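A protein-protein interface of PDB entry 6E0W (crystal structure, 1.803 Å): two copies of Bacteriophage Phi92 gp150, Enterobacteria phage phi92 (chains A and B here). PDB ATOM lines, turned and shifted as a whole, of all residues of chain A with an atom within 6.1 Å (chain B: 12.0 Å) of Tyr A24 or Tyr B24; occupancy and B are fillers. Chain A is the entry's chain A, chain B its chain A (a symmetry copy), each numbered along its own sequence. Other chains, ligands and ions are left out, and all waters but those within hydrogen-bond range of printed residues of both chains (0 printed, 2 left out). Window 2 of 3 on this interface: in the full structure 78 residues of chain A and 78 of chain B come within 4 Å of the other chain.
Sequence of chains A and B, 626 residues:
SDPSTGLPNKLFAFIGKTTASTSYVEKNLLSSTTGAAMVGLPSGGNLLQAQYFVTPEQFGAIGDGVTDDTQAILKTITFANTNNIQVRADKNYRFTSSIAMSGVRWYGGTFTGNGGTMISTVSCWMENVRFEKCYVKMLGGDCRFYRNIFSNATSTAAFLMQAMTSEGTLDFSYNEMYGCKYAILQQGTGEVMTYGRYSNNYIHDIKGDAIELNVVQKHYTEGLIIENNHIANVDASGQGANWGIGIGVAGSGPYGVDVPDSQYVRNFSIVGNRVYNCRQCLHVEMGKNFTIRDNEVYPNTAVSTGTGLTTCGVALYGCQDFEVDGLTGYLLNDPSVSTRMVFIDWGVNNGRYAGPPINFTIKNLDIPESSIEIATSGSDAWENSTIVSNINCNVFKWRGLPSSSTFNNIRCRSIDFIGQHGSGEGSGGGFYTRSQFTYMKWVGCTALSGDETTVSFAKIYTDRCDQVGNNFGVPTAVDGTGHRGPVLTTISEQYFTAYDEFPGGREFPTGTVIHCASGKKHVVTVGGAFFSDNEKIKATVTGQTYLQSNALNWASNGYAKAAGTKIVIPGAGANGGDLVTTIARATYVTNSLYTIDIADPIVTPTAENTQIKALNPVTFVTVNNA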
ATOM      1  N   SER A  23     -15.522  29.692 -33.652  1.00  0.00           N
ATOM      2  CA  SER A  23     -15.660  30.468 -32.426  1.00  0.00           C
ATOM      3  C   SER A  23     -15.678  29.510 -31.243  1.00  0.00           C
ATOM      4  O   SER A  23     -16.180  29.830 -30.162  1.00  0.00           O
ATOM      5  CB  SER A  23     -16.930  31.321 -32.467  1.00  0.00           C
ATOM      6  OG  SER A  23     -17.014  32.171 -31.339  1.00  0.00           O
ATOM      7  N   TYR A  24     -15.118  28.324 -31.477  1.00  0.00           N
ATOM      8  CA  TYR A  24     -15.141  27.210 -30.540  1.00  0.00           C
ATOM      9  C   TYR A  24     -13.709  26.854 -30.151  1.00  0.00           C
ATOM     10  O   TYR A  24     -12.766  27.116 -30.903  1.00  0.00           O
ATOM     11  CB  TYR A  24     -15.849  25.973 -31.153  1.00  0.00           C
ATOM     12  CG  TYR A  24     -17.329  26.125 -31.508  1.00  0.00           C
ATOM     13  CD1 TYR A  24     -18.048  27.270 -31.172  1.00  0.00           C
ATOM     14  CD2 TYR A  24     -18.009  25.100 -32.163  1.00  0.00           C
ATOM     15  CE1 TYR A  24     -19.396  27.396 -31.496  1.00  0.00           C
ATOM     16  CE2 TYR A  24     -19.356  25.215 -32.487  1.00  0.00           C
ATOM     17  CZ  TYR A  24     -20.044  26.364 -32.152  1.00  0.00           C
ATOM     18  OH  TYR A  24     -21.380  26.480 -32.472  1.00  0.00           O
ATOM     19  N   VAL A  25     -13.540  26.250 -28.971  1.00  0.00           N
ATOM     20  CA  VAL A  25     -12.200  25.915 -28.505  1.00  0.00           C
ATOM     21  C   VAL A  25     -11.654  24.766 -29.339  1.00  0.00           C
ATOM     22  O   VAL A  25     -12.389  23.863 -29.750  1.00  0.00           O
ATOM     23  CB  VAL A  25     -12.167  25.567 -27.002  1.00  0.00           C
ATOM     24  CG1 VAL A  25     -12.745  26.683 -26.160  1.00  0.00           C
ATOM     25  CG2 VAL A  25     -12.852  24.235 -26.702  1.00  0.00           C
ATOM     26  N   GLU A  26     -10.367  24.830 -29.644  1.00  0.00           N
ATOM     27  CA  GLU A  26      -9.712  23.778 -30.401  1.00  0.00           C
ATOM     28  C   GLU A  26      -9.433  22.569 -29.523  1.00  0.00           C
ATOM     29  O   GLU A  26      -9.274  22.687 -28.305  1.00  0.00           O
ATOM     30  CB  GLU A  26      -8.387  24.269 -30.976  1.00  0.00           C
ATOM     31  CG  GLU A  26      -8.503  25.313 -32.053  1.00  0.00           C
ATOM     32  CD  GLU A  26      -7.157  25.900 -32.387  1.00  0.00           C
ATOM     33  OE1 GLU A  26      -7.091  27.102 -32.707  1.00  0.00           O
ATOM     34  OE2 GLU A  26      -6.157  25.157 -32.303  1.00  0.00           O
ATOM     35  N   LYS A  27      -9.437  21.388 -30.144  1.00  0.00           N
ATOM     36  CA  LYS A  27      -9.053  20.181 -29.417  1.00  0.00           C
ATOM     37  C   LYS A  27      -7.651  20.347 -28.849  1.00  0.00           C
ATOM     38  O   LYS A  27      -7.408  20.093 -27.662  1.00  0.00           O
ATOM     39  CB  LYS A  27      -9.143  18.961 -30.336  1.00  0.00           C
ATOM     40  CG  LYS A  27      -8.099  17.883 -30.088  1.00  0.00           C
ATOM     41  CD  LYS A  27      -8.195  16.788 -31.146  1.00  0.00           C
ATOM     42  CE  LYS A  27      -6.931  15.953 -31.197  1.00  0.00           C
ATOM     43  NZ  LYS A  27      -6.485  15.581 -29.827  1.00  0.00           N
ATOM     44  N   SER B  23     -11.845  19.766 -35.825  1.00  0.00           N
ATOM     45  CA  SER B  23     -10.588  19.614 -35.105  1.00  0.00           C
ATOM     46  C   SER B  23     -10.756  20.191 -33.706  1.00  0.00           C
ATOM     47  O   SER B  23      -9.785  20.564 -33.041  1.00  0.00           O
ATOM     48  CB  SER B  23      -9.448  20.306 -35.855  1.00  0.00           C
ATOM     49  OG  SER B  23      -8.201  20.063 -35.233  1.00  0.00           O
ATOM     50  N   TYR B  24     -12.016  20.256 -33.277  1.00  0.00           N
ATOM     51  CA  TYR B  24     -12.423  20.891 -32.032  1.00  0.00           C
ATOM     52  C   TYR B  24     -13.067  19.847 -31.125  1.00  0.00           C
ATOM     53  O   TYR B  24     -13.593  18.835 -31.598  1.00  0.00           O
ATOM     54  CB  TYR B  24     -13.416  22.055 -32.293  1.00  0.00           C
ATOM     55  CG  TYR B  24     -12.897  23.242 -33.105  1.00  0.00           C
ATOM     56  CD1 TYR B  24     -11.559  23.344 -33.478  1.00  0.00           C
ATOM     57  CD2 TYR B  24     -13.756  24.274 -33.477  1.00  0.00           C
ATOM     58  CE1 TYR B  24     -11.096  24.432 -34.214  1.00  0.00           C
ATOM     59  CE2 TYR B  24     -13.302  25.366 -34.208  1.00  0.00           C
ATOM     60  CZ  TYR B  24     -11.972  25.440 -34.574  1.00  0.00           C
ATOM     61  OH  TYR B  24     -11.520  26.523 -35.298  1.00  0.00           O
ATOM     62  N   VAL B  25     -13.031  20.091 -29.811  1.00  0.00           N
ATOM     63  CA  VAL B  25     -13.586  19.123 -28.872  1.00  0.00           C
ATOM     64  C   VAL B  25     -15.103  19.131 -28.983  1.00  0.00           C
ATOM     65  O   VAL B  25     -15.725  20.173 -29.207  1.00  0.00           O
ATOM     66  CB  VAL B  25     -13.140  19.387 -27.419  1.00  0.00           C
ATOM     67  CG1 VAL B  25     -11.632  19.422 -27.297  1.00  0.00           C
ATOM     68  CG2 VAL B  25     -13.771  20.652 -26.841  1.00  0.00           C
ATOM     69  N   GLU B  26     -15.699  17.953 -28.887  1.00  0.00           N
ATOM     70  CA  GLU B  26     -17.145  17.826 -28.937  1.00  0.00           C
ATOM     71  C   GLU B  26     -17.773  18.240 -27.615  1.00  0.00           C
ATOM     72  O   GLU B  26     -17.149  18.146 -26.554  1.00  0.00           O
ATOM     73  CB  GLU B  26     -17.553  16.387 -29.231  1.00  0.00           C
ATOM     74  CG  GLU B  26     -17.214  15.894 -30.612  1.00  0.00           C
ATOM     75  CD  GLU B  26     -17.438  14.409 -30.729  1.00  0.00           C
ATOM     76  OE1 GLU B  26     -16.678  13.745 -31.458  1.00  0.00           O
ATOM     77  OE2 GLU B  26     -18.366  13.903 -30.064  1.00  0.00           O
ATOM     78  N   LYS B  27     -18.999  18.761 -27.694  1.00  0.00           N
ATOM     79  CA  LYS B  27     -19.739  19.070 -26.474  1.00  0.00           C
ATOM     80  C   LYS B  27     -19.875  17.815 -25.624  1.00  0.00           C
ATOM     81  O   LYS B  27     -19.591  17.825 -24.419  1.00  0.00           O
ATOM     82  CB  LYS B  27     -21.106  19.660 -26.822  1.00  0.00           C
ATOM     83  CG  LYS B  27     -22.235  19.292 -25.870  1.00  0.00           C
ATOM     84  CD  LYS B  27     -23.570  19.816 -26.390  1.00  0.00           C
ATOM     85  CE  LYS B  27     -24.737  19.112 -25.727  1.00  0.00           C
ATOM     86  NZ  LYS B  27     -24.535  19.017 -24.257  1.00  0.00           N
ATOM     87  N   ASN B  28     -20.274  16.711 -26.249  1.00  0.00           N
ATOM     88  CA  ASN B  28     -20.297  15.427 -25.577  1.00  0.00           C
ATOM     89  C   ASN B  28     -18.858  14.985 -25.339  1.00  0.00           C
ATOM     90  O   ASN B  28     -17.908  15.688 -25.694  1.00  0.00           O
ATOM     91  CB  ASN B  28     -21.083  14.425 -26.412  1.00  0.00           C
ATOM     92  CG  ASN B  28     -22.499  14.890 -26.662  1.00  0.00           C
ATOM     93  OD1 ASN B  28     -23.158  15.402 -25.755  1.00  0.00           O
ATOM     94  ND2 ASN B  28     -22.954  14.776 -27.905  1.00  0.00           N
ATOM     95  N   LEU B  29     -18.683  13.821 -24.718  1.00  0.00           N
ATOM     96  CA  LEU B  29     -17.348  13.295 -24.440  1.00  0.00           C
ATOM     97  C   LEU B  29     -16.623  14.169 -23.411  1.00  0.00           C
ATOM     98  O   LEU B  29     -16.053  13.641 -22.450  1.00  0.00           O
ATOM     99  CB  LEU B  29     -16.522  13.173 -25.728  1.00  0.00           C
ATOM    100  CG  LEU B  29     -17.016  12.207 -26.800  1.00  0.00           C
ATOM    101  CD1 LEU B  29     -16.096  12.261 -28.002  1.00  0.00           C
ATOM    102  CD2 LEU B  29     -17.089  10.795 -26.245  1.00  0.00           C
ATOM    103  N   LEU B  30     -16.608  15.498 -23.611  1.00  0.00           N
ATOM    104  CA  LEU B  30     -16.067  16.388 -22.584  1.00  0.00           C
ATOM    105  C   LEU B  30     -16.896  16.299 -21.310  1.00  0.00           C
ATOM    106  O   LEU B  30     -16.367  16.484 -20.209  1.00  0.00           O
ATOM    107  CB  LEU B  30     -16.008  17.843 -23.073  1.00  0.00           C
ATOM    108  CG  LEU B  30     -15.285  18.818 -22.114  1.00  0.00           C
ATOM    109  CD1 LEU B  30     -13.785  18.557 -22.086  1.00  0.00           C
ATOM    110  CD2 LEU B  30     -15.561  20.289 -22.405  1.00  0.00           C
ATOM    111  N   SER B  31     -18.193  16.033 -21.438  1.00  0.00           N
ATOM    112  CA  SER B  31     -19.034  15.817 -20.269  1.00  0.00           C
ATOM    113  C   SER B  31     -18.981  14.377 -19.765  1.00  0.00           C
ATOM    114  O   SER B  31     -19.525  14.093 -18.691  1.00  0.00           O
ATOM    115  CB  SER B  31     -20.481  16.206 -20.594  1.00  0.00           C
ATOM    116  OG  SER B  31     -21.016  15.390 -21.616  1.00  0.00           O
ATOM    117  N   GLY B  35     -13.967  13.070 -19.612  1.00  0.00           N
ATOM    118  CA  GLY B  35     -13.817  14.377 -20.229  1.00  0.00           C
ATOM    119  C   GLY B  35     -12.633  15.171 -19.719  1.00  0.00           C
ATOM    120  O   GLY B  35     -11.975  15.870 -20.496  1.00  0.00           O
ATOM    121  N   MET B  38      -9.132  15.622 -21.377  1.00  0.00           N
ATOM    122  CA  MET B  38      -8.855  16.511 -22.500  1.00  0.00           C
ATOM    123  C   MET B  38      -8.168  17.817 -22.106  1.00  0.00           C
ATOM    124  O   MET B  38      -7.712  18.542 -22.997  1.00  0.00           O
ATOM    125  CB  MET B  38     -10.155  16.840 -23.242  1.00  0.00           C
ATOM    126  CG  MET B  38     -10.932  15.621 -23.717  1.00  0.00           C
ATOM    127  SD  MET B  38     -12.419  16.066 -24.646  1.00  0.00           S
ATOM    128  CE  MET B  38     -13.359  14.542 -24.550  1.00  0.00           C
ATOM    129  N   VAL B  39      -8.057  18.131 -20.819  1.00  0.00           N
ATOM    130  CA  VAL B  39      -7.606  19.448 -20.381  1.00  0.00           C
ATOM    131  C   VAL B  39      -6.163  19.361 -19.915  1.00  0.00           C
ATOM    132  O   VAL B  39      -5.845  18.585 -19.009  1.00  0.00           O
ATOM    133  CB  VAL B  39      -8.501  20.002 -19.264  1.00  0.00           C
ATOM    134  CG1 VAL B  39      -8.045  21.410 -18.864  1.00  0.00           C
ATOM    135  CG2 VAL B  39      -9.947  19.989 -19.697  1.00  0.00           C
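The backbone carbonyl oxygen (O) of Ser B23 lies within hydrogen-bond range of the backbone NH (N) of Lys A27 (3.0 Å).
Tyr A24 touches just one residue of chain B: Tyr B24 (3.6 Å).
No residue of chain B comes within 4 Å of Ser A23.
Printed residues of chain B within 4 Å of Glu A26: Tyr B24 (3.5 Å).
Of the printed residues of chain B, Lys A27 touches Ser B23 (3.0 Å), Tyr B24 (3.6 Å) and Val B25 (3.4 Å).
Of the printed residues of chain A, Val B25 touches Val A25 and Lys A27.
Printed residues of chain A within 4 Å of Ser B23: Lys A27 (3.0 Å).
Leu B29 touches none of the printed residues of chain A.
The nearest residue of chain B that does not touch Tyr A24 is Val B25 (6.1 Å).
The nearest residue of chain A that does not touch Tyr B24 is Ser A23 (4.9 Å).
The nearest printed residue of chain A that does not touch Val B25 is Glu A26 (4.2 Å).
Tyr A24 touches Tyr B24 (CB to CD2, 3.6 Å).
Val A25 touches Tyr B24.
Val A25 touches Val B25 (CG2 to CG2, 3.7 Å).
CE1 of Tyr B24 touches CG of Glu A26, 3.5 Å away.
Tyr B24 touches Lys A27 (CA to N, 3.6 Å).
CA of Lys A27 touches CG1 of Val B25 (3.4 Å).
Of the 5 printed residues of chain A, 4 touch a printed residue of chain B.
Hydrophobic or aromatic side chains of chain A within 4 Å of the printed part of chain B: Tyr A24 and Val A25.
Among the printed residues, no Asp or Glu carboxylate lies within 4 Å of a Lys or Arg side-chain nitrogen of the other chain.
Tyr A24 touches its own counterpart, Tyr B24.
Val A25 touches Tyr B24, but with the chains exchanged Tyr A24 does not touch Val B25 (6.1 Å).
Val A25 touches its own counterpart, Val B25.
Lys A27 touches Ser B23, but with the chains exchanged Ser A23 does not touch Lys B27 (11.7 Å).
Positions printed for both chains: 23, 24, 25, 26 and 27.
Of the 7 pairs that touch across the chains among the printed residues, 2 have their exchanged pair printed and touching as well.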
